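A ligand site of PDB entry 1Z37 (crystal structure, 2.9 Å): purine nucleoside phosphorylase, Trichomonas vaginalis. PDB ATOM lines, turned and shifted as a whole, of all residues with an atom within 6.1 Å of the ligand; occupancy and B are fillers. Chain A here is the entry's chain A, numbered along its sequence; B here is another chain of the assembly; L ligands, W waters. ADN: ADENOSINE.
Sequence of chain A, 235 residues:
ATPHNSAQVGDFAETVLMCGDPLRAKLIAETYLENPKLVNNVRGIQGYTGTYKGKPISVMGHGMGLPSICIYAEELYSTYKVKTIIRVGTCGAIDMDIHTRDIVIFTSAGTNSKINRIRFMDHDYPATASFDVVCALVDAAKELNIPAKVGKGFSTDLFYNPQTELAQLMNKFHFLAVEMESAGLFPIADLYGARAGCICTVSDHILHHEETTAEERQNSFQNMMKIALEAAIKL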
ATOM      1  N   GLY A  20      19.847   5.089   2.335  1.00  0.00           N
ATOM      2  CA  GLY A  20      20.972   5.032   1.415  1.00  0.00           C
ATOM      3  C   GLY A  20      21.456   3.626   1.119  1.00  0.00           C
ATOM      4  O   GLY A  20      21.596   3.235  -0.036  1.00  0.00           O
ATOM      5  N   ASP A  21      21.685   2.862   2.187  1.00  0.00           N
ATOM      6  CA  ASP A  21      22.193   1.505   2.084  1.00  0.00           C
ATOM      7  C   ASP A  21      21.173   0.490   1.548  1.00  0.00           C
ATOM      8  O   ASP A  21      20.106   0.291   2.131  1.00  0.00           O
ATOM      9  CB  ASP A  21      22.689   1.063   3.457  1.00  0.00           C
ATOM     10  CG  ASP A  21      23.499  -0.190   3.393  1.00  0.00           C
ATOM     11  OD1 ASP A  21      23.116  -1.094   2.628  1.00  0.00           O
ATOM     12  OD2 ASP A  21      24.502  -0.284   4.131  1.00  0.00           O
ATOM     13  N   HIS A  62      18.311   4.184  -1.956  1.00  0.00           N
ATOM     14  CA  HIS A  62      18.303   5.375  -2.809  1.00  0.00           C
ATOM     15  C   HIS A  62      19.690   5.930  -3.075  1.00  0.00           C
ATOM     16  O   HIS A  62      19.821   6.985  -3.687  1.00  0.00           O
ATOM     17  CB  HIS A  62      17.400   6.474  -2.209  1.00  0.00           C
ATOM     18  CG  HIS A  62      17.852   6.991  -0.872  1.00  0.00           C
ATOM     19  ND1 HIS A  62      19.144   7.376  -0.614  1.00  0.00           N
ATOM     20  CD2 HIS A  62      17.154   7.202   0.274  1.00  0.00           C
ATOM     21  CE1 HIS A  62      19.238   7.815   0.630  1.00  0.00           C
ATOM     22  NE2 HIS A  62      18.043   7.720   1.188  1.00  0.00           N
ATOM     23  N   GLY A  63      20.712   5.217  -2.629  1.00  0.00           N
ATOM     24  CA  GLY A  63      22.076   5.664  -2.852  1.00  0.00           C
ATOM     25  C   GLY A  63      22.457   6.856  -1.996  1.00  0.00           C
ATOM     26  O   GLY A  63      21.777   7.193  -1.044  1.00  0.00           O
ATOM     27  N   MET A  64      23.570   7.495  -2.332  1.00  0.00           N
ATOM     28  CA  MET A  64      24.028   8.630  -1.566  1.00  0.00           C
ATOM     29  C   MET A  64      24.055   9.885  -2.409  1.00  0.00           C
ATOM     30  O   MET A  64      24.545   9.857  -3.537  1.00  0.00           O
ATOM     31  CB  MET A  64      25.432   8.379  -1.028  1.00  0.00           C
ATOM     32  CG  MET A  64      25.583   7.113  -0.205  1.00  0.00           C
ATOM     33  SD  MET A  64      27.228   6.993   0.526  1.00  0.00           S
ATOM     34  CE  MET A  64      28.169   6.488  -0.896  1.00  0.00           C
ATOM     35  N   GLY A  65      23.519  10.973  -1.865  1.00  0.00           N
ATOM     36  CA  GLY A  65      23.500  12.231  -2.574  1.00  0.00           C
ATOM     37  C   GLY A  65      22.209  12.609  -3.260  1.00  0.00           C
ATOM     38  O   GLY A  65      21.425  11.753  -3.669  1.00  0.00           O
ATOM     39  N   ARG A  87      12.105   9.015   4.294  1.00  0.00           N
ATOM     40  CA  ARG A  87      13.525   8.705   4.270  1.00  0.00           C
ATOM     41  C   ARG A  87      13.987   8.318   5.677  1.00  0.00           C
ATOM     42  O   ARG A  87      13.888   9.102   6.619  1.00  0.00           O
ATOM     43  CB  ARG A  87      14.312   9.911   3.766  1.00  0.00           C
ATOM     44  CG  ARG A  87      15.612   9.543   3.061  1.00  0.00           C
ATOM     45  CD  ARG A  87      16.547  10.738   2.899  1.00  0.00           C
ATOM     46  NE  ARG A  87      17.501  10.839   4.001  1.00  0.00           N
ATOM     47  CZ  ARG A  87      18.364   9.873   4.343  1.00  0.00           C
ATOM     48  NH1 ARG A  87      18.380   8.726   3.680  1.00  0.00           N
ATOM     49  NH2 ARG A  87      19.212  10.074   5.340  1.00  0.00           N
ATOM     50  N   THR A  90      20.780   7.320   8.633  1.00  0.00           N
ATOM     51  CA  THR A  90      21.707   7.877   9.602  1.00  0.00           C
ATOM     52  C   THR A  90      22.027   9.306   9.214  1.00  0.00           C
ATOM     53  O   THR A  90      21.609   9.775   8.165  1.00  0.00           O
ATOM     54  CB  THR A  90      23.014   7.104   9.649  1.00  0.00           C
ATOM     55  OG1 THR A  90      23.513   6.945   8.313  1.00  0.00           O
ATOM     56  CG2 THR A  90      22.807   5.742  10.289  1.00  0.00           C
ATOM     57  N   CYS A  91      22.789   9.979  10.068  1.00  0.00           N
ATOM     58  CA  CYS A  91      23.169  11.348   9.808  1.00  0.00           C
ATOM     59  C   CYS A  91      24.214  11.783  10.813  1.00  0.00           C
ATOM     60  O   CYS A  91      24.551  11.033  11.744  1.00  0.00           O
ATOM     61  CB  CYS A  91      21.938  12.257   9.916  1.00  0.00           C
ATOM     62  SG  CYS A  91      21.081  12.186  11.513  1.00  0.00           S
ATOM     63  N   GLY A  92      24.735  12.990  10.633  1.00  0.00           N
ATOM     64  CA  GLY A  92      25.714  13.509  11.543  1.00  0.00           C
ATOM     65  C   GLY A  92      25.131  14.654  12.366  1.00  0.00           C
ATOM     66  O   GLY A  92      24.545  15.589  11.816  1.00  0.00           O
ATOM     67  N   ALA A  93      25.270  14.579  13.683  1.00  0.00           N
ATOM     68  CA  ALA A  93      24.767  15.638  14.549  1.00  0.00           C
ATOM     69  C   ALA A  93      25.596  16.881  14.315  1.00  0.00           C
ATOM     70  O   ALA A  93      26.794  16.785  14.078  1.00  0.00           O
ATOM     71  CB  ALA A  93      24.851  15.206  16.019  1.00  0.00           C
ATOM     72  N   THR A 156      24.193  17.695   2.429  1.00  0.00           N
ATOM     73  CA  THR A 156      25.471  18.130   1.881  1.00  0.00           C
ATOM     74  C   THR A 156      25.807  17.393   0.591  1.00  0.00           C
ATOM     75  O   THR A 156      25.433  16.237   0.418  1.00  0.00           O
ATOM     76  CB  THR A 156      26.626  17.904   2.889  1.00  0.00           C
ATOM     77  OG1 THR A 156      27.842  18.444   2.365  1.00  0.00           O
ATOM     78  CG2 THR A 156      26.812  16.407   3.154  1.00  0.00           C
ATOM     79  N   LEU A 158      28.964  17.510  -0.284  1.00  0.00           N
ATOM     80  CA  LEU A 158      30.304  17.098   0.128  1.00  0.00           C
ATOM     81  C   LEU A 158      30.278  16.395   1.490  1.00  0.00           C
ATOM     82  O   LEU A 158      30.181  17.054   2.525  1.00  0.00           O
ATOM     83  CB  LEU A 158      31.248  18.322   0.219  1.00  0.00           C
ATOM     84  CG  LEU A 158      32.007  18.968  -0.950  1.00  0.00           C
ATOM     85  CD1 LEU A 158      32.309  17.924  -2.009  1.00  0.00           C
ATOM     86  CD2 LEU A 158      31.208  20.108  -1.541  1.00  0.00           C
ATOM     87  N   PHE A 159      30.336  15.067   1.501  1.00  0.00           N
ATOM     88  CA  PHE A 159      30.378  14.342   2.765  1.00  0.00           C
ATOM     89  C   PHE A 159      31.621  14.891   3.490  1.00  0.00           C
ATOM     90  O   PHE A 159      31.562  15.293   4.649  1.00  0.00           O
ATOM     91  CB  PHE A 159      30.550  12.852   2.522  1.00  0.00           C
ATOM     92  CG  PHE A 159      30.718  12.056   3.786  1.00  0.00           C
ATOM     93  CD1 PHE A 159      29.612  11.480   4.416  1.00  0.00           C
ATOM     94  CD2 PHE A 159      31.978  11.872   4.347  1.00  0.00           C
ATOM     95  CE1 PHE A 159      29.764  10.738   5.583  1.00  0.00           C
ATOM     96  CE2 PHE A 159      32.139  11.130   5.513  1.00  0.00           C
ATOM     97  CZ  PHE A 159      31.042  10.559   6.134  1.00  0.00           C
ATOM     98  N   VAL A 178      23.157  16.479   9.674  1.00  0.00           N
ATOM     99  CA  VAL A 178      23.481  16.576   8.257  1.00  0.00           C
ATOM    100  C   VAL A 178      23.463  15.203   7.594  1.00  0.00           C
ATOM    101  O   VAL A 178      23.964  14.222   8.138  1.00  0.00           O
ATOM    102  CB  VAL A 178      24.880  17.215   8.045  1.00  0.00           C
ATOM    103  CG1 VAL A 178      25.938  16.457   8.850  1.00  0.00           C
ATOM    104  CG2 VAL A 178      25.242  17.191   6.580  1.00  0.00           C
ATOM    105  N   GLU A 179      22.846  15.140   6.413  1.00  0.00           N
ATOM    106  CA  GLU A 179      22.803  13.897   5.638  1.00  0.00           C
ATOM    107  C   GLU A 179      23.087  14.247   4.170  1.00  0.00           C
ATOM    108  O   GLU A 179      23.834  15.191   3.907  1.00  0.00           O
ATOM    109  CB  GLU A 179      21.457  13.168   5.825  1.00  0.00           C
ATOM    110  CG  GLU A 179      20.247  14.050   5.962  1.00  0.00           C
ATOM    111  CD  GLU A 179      19.552  14.280   4.636  1.00  0.00           C
ATOM    112  OE1 GLU A 179      19.298  15.452   4.307  1.00  0.00           O
ATOM    113  OE2 GLU A 179      19.242  13.296   3.943  1.00  0.00           O
ATOM    114  N   MET A 180      22.523  13.503   3.222  1.00  0.00           N
ATOM    115  CA  MET A 180      22.802  13.817   1.816  1.00  0.00           C
ATOM    116  C   MET A 180      21.670  13.574   0.828  1.00  0.00           C
ATOM    117  O   MET A 180      21.940  13.352  -0.353  1.00  0.00           O
ATOM    118  CB  MET A 180      24.009  12.996   1.343  1.00  0.00           C
ATOM    119  CG  MET A 180      25.323  13.388   1.977  1.00  0.00           C
ATOM    120  SD  MET A 180      26.717  12.337   1.515  1.00  0.00           S
ATOM    121  CE  MET A 180      26.876  12.768  -0.227  1.00  0.00           C
ATOM    122  N   GLU A 181      20.421  13.624   1.262  1.00  0.00           N
ATOM    123  CA  GLU A 181      19.333  13.343   0.332  1.00  0.00           C
ATOM    124  C   GLU A 181      18.051  14.159   0.484  1.00  0.00           C
ATOM    125  O   GLU A 181      17.454  14.579  -0.516  1.00  0.00           O
ATOM    126  CB  GLU A 181      18.982  11.855   0.379  1.00  0.00           C
ATOM    127  CG  GLU A 181      20.109  10.898  -0.005  1.00  0.00           C
ATOM    128  CD  GLU A 181      21.133  10.647   1.106  1.00  0.00           C
ATOM    129  OE1 GLU A 181      22.237  10.116   0.821  1.00  0.00           O
ATOM    130  OE2 GLU A 181      20.828  10.970   2.281  1.00  0.00           O
ATOM    131  N   SER A 203      24.204   8.870  13.778  1.00  0.00           N
ATOM    132  CA  SER A 203      25.263   7.869  13.901  1.00  0.00           C
ATOM    133  C   SER A 203      26.542   8.455  14.474  1.00  0.00           C
ATOM    134  O   SER A 203      27.416   7.733  14.961  1.00  0.00           O
ATOM    135  CB  SER A 203      25.548   7.227  12.549  1.00  0.00           C
ATOM    136  OG  SER A 203      25.897   8.209  11.583  1.00  0.00           O
ATOM    137  N   ASP A 204      26.669   9.774  14.407  1.00  0.00           N
ATOM    138  CA  ASP A 204      27.849  10.433  14.956  1.00  0.00           C
ATOM    139  C   ASP A 204      27.666  11.936  14.991  1.00  0.00           C
ATOM    140  O   ASP A 204      26.701  12.470  14.436  1.00  0.00           O
ATOM    141  CB  ASP A 204      29.088  10.070  14.143  1.00  0.00           C
ATOM    142  CG  ASP A 204      30.380  10.492  14.841  1.00  0.00           C
ATOM    143  OD1 ASP A 204      30.514  10.197  16.046  1.00  0.00           O
ATOM    144  OD2 ASP A 204      31.243  11.105  14.178  1.00  0.00           O
ATOM    145  N   ILE A 206      29.521  15.576  14.180  1.00  0.00           N
ATOM    146  CA  ILE A 206      30.614  16.167  13.422  1.00  0.00           C
ATOM    147  C   ILE A 206      31.431  17.187  14.216  1.00  0.00           C
ATOM    148  O   ILE A 206      32.633  17.347  13.966  1.00  0.00           O
ATOM    149  CB  ILE A 206      30.120  16.838  12.116  1.00  0.00           C
ATOM    150  CG1 ILE A 206      29.390  18.144  12.423  1.00  0.00           C
ATOM    151  CG2 ILE A 206      29.219  15.875  11.346  1.00  0.00           C
ATOM    152  CD1 ILE A 206      28.938  18.885  11.183  1.00  0.00           C
ATOM    153  N   PRO B   3      33.804   4.914   6.720  1.00  0.00           N
ATOM    154  CA  PRO B   3      32.365   4.767   6.919  1.00  0.00           C
ATOM    155  C   PRO B   3      31.689   4.114   5.730  1.00  0.00           C
ATOM    156  O   PRO B   3      30.504   3.768   5.792  1.00  0.00           O
ATOM    157  CB  PRO B   3      31.891   6.216   7.093  1.00  0.00           C
ATOM    158  CG  PRO B   3      33.096   6.919   7.663  1.00  0.00           C
ATOM    159  CD  PRO B   3      34.207   6.324   6.826  1.00  0.00           C
ATOM    160  N   HIS B   4      32.425   3.950   4.631  1.00  0.00           N
ATOM    161  CA  HIS B   4      31.861   3.366   3.415  1.00  0.00           C
ATOM    162  C   HIS B   4      32.727   2.259   2.849  1.00  0.00           C
ATOM    163  O   HIS B   4      32.475   1.767   1.751  1.00  0.00           O
ATOM    164  CB  HIS B   4      31.692   4.456   2.348  1.00  0.00           C
ATOM    165  CG  HIS B   4      31.083   5.722   2.859  1.00  0.00           C
ATOM    166  ND1 HIS B   4      31.788   6.636   3.614  1.00  0.00           N
ATOM    167  CD2 HIS B   4      29.822   6.209   2.759  1.00  0.00           C
ATOM    168  CE1 HIS B   4      30.982   7.623   3.965  1.00  0.00           C
ATOM    169  NE2 HIS B   4      29.791   7.388   3.449  1.00  0.00           N
ATOM    170  N   ARG B  43      27.427  -1.122   2.056  1.00  0.00           N
ATOM    171  CA  ARG B  43      26.379  -0.577   1.195  1.00  0.00           C
ATOM    172  C   ARG B  43      26.347  -1.341  -0.121  1.00  0.00           C
ATOM    173  O   ARG B  43      26.097  -0.760  -1.180  1.00  0.00           O
ATOM    174  CB  ARG B  43      26.617   0.907   0.946  1.00  0.00           C
ATOM    175  CG  ARG B  43      26.415   1.761   2.193  1.00  0.00           C
ATOM    176  CD  ARG B  43      26.936   3.173   1.998  1.00  0.00           C
ATOM    177  NE  ARG B  43      26.664   4.034   3.153  1.00  0.00           N
ATOM    178  CZ  ARG B  43      25.509   4.641   3.399  1.00  0.00           C
ATOM    179  NH1 ARG B  43      24.481   4.496   2.561  1.00  0.00           N
ATOM    180  NH2 ARG B  43      25.374   5.394   4.485  1.00  0.00           N
ATOM    181  N   ILE B  71      32.732  10.557  -2.356  1.00  0.00           N
ATOM    182  CA  ILE B  71      33.015   9.936  -1.075  1.00  0.00           C
ATOM    183  C   ILE B  71      34.047   8.835  -1.324  1.00  0.00           C
ATOM    184  O   ILE B  71      35.128   8.833  -0.748  1.00  0.00           O
ATOM    185  CB  ILE B  71      31.724   9.346  -0.458  1.00  0.00           C
ATOM    186  CG1 ILE B  71      30.648  10.434  -0.331  1.00  0.00           C
ATOM    187  CG2 ILE B  71      32.013   8.794   0.930  1.00  0.00           C
ATOM    188  CD1 ILE B  71      29.331   9.969   0.246  1.00  0.00           C
HETATM  189  O5' ADN L   1      27.710   8.434   4.551  1.00  0.00           O
HETATM  190  C5' ADN L   1      26.786   9.316   3.888  1.00  0.00           C
HETATM  191  C4' ADN L   1      25.445   8.604   3.743  1.00  0.00           C
HETATM  192  O4' ADN L   1      24.852   8.320   5.026  1.00  0.00           O
HETATM  193  C3' ADN L   1      24.367   9.457   3.066  1.00  0.00           C
HETATM  194  O3' ADN L   1      23.262   8.638   2.655  1.00  0.00           O
HETATM  195  C2' ADN L   1      23.947  10.375   4.224  1.00  0.00           C
HETATM  196  O2' ADN L   1      22.588  10.779   4.102  1.00  0.00           O
HETATM  197  C1' ADN L   1      24.180   9.510   5.467  1.00  0.00           C
HETATM  198  N9  ADN L   1      24.955  10.187   6.541  1.00  0.00           N
HETATM  199  C8  ADN L   1      25.091   9.711   7.781  1.00  0.00           C
HETATM  200  N7  ADN L   1      25.884  10.515   8.480  1.00  0.00           N
HETATM  201  C5  ADN L   1      26.263  11.509   7.689  1.00  0.00           C
HETATM  202  C6  ADN L   1      27.115  12.595   7.842  1.00  0.00           C
HETATM  203  N6  ADN L   1      27.711  12.829   9.008  1.00  0.00           N
HETATM  204  N1  ADN L   1      27.333  13.410   6.789  1.00  0.00           N
HETATM  205  C2  ADN L   1      26.738  13.190   5.622  1.00  0.00           C
HETATM  206  N3  ADN L   1      25.918  12.164   5.451  1.00  0.00           N
HETATM  207  C4  ADN L   1      25.661  11.310   6.449  1.00  0.00           C
HETATM  208  O   HOH W   1      27.894   6.513   6.875  1.00  0.00           O
HETATM  209  O   HOH W   2      29.360  15.842   6.399  1.00  0.00           O
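Met 64 touches the ligand (CG to O3', 3.99 Å).
Arg 87 touches the ligand (NH2 to O2', 3.7 Å).
Thr 90 touches the ligand (OG1 to C8, 3.2 Å).
Cys 91 touches the ligand (CA to N7, 3.1 Å).
Phe 159 touches the ligand (CE1 to O5', 3.3 Å).
O of Val 178 touches C6 of the ligand, 3.6 Å away.
CB of Glu 179 touches O2' of the ligand (3.2 Å).
OG of Ser 203 touches N7 of the ligand, at 3.9 Å.
Hydrophobic or aromatic side chains that line the ligand: Met 64, Phe 159, Val 178, Met 180 and His 4 of chain B.
Of the 25 residues printed, 13 come within 4 Å of the ligand.
The nearest printed residue that does not touch the ligand is Thr 156 (4.1 Å).
The backbone NH (N) of Met 180 lies within hydrogen-bond range of an oxygen (O2') of the ligand (2.9 Å).
N7 of the ligand lies within hydrogen-bond range of N of Gly 92 (3.5 Å).
O5' of the ligand is in hydrogen-bond range of NE2 of His 4 of chain B.
An oxygen (O2') of the ligand is in hydrogen-bond range of the side-chain carboxylate of Glu 181, 2.5 Å away.
An oxygen (O4') of the ligand sits at hydrogen-bond distance from the guanidinium group (NH2) of Arg 43 of chain B.
The backbone carbonyl oxygen (O) of Gly 92 is in hydrogen-bond range of the backbone NH (N) of Val 178 (2.7 Å).
NH1 of Arg 87 lies within hydrogen-bond range of NE2 of His 62 (2.7 Å).
The backbone carbonyl oxygen of Cys 91 sits at hydrogen-bond distance from the backbone NH of Ser 203, 3.0 Å away.
The backbone NH of Gly 65 sits close to the backbone carbonyl oxygen of Met 180 (3.2 Å).
The backbone carbonyl oxygen (O) of Glu 179 lies within hydrogen-bond range of the backbone NH (N) of Thr 156, at 2.9 Å.
N of Glu 181 sits at hydrogen-bond distance from OE2 of Glu 179 (2.9 Å).
The guanidinium group (NH2) of Arg 87 is in salt-bridge range of the side-chain carboxylate (OE2) of Glu 181 (3.6 Å).
OE1 of Glu 181 lies within hydrogen-bond range of N of Gly 65 (3.1 Å).
Water W2 lies within hydrogen-bond range of O of Phe 159 (2.9 Å) and N1 of the ligand (3.2 Å).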
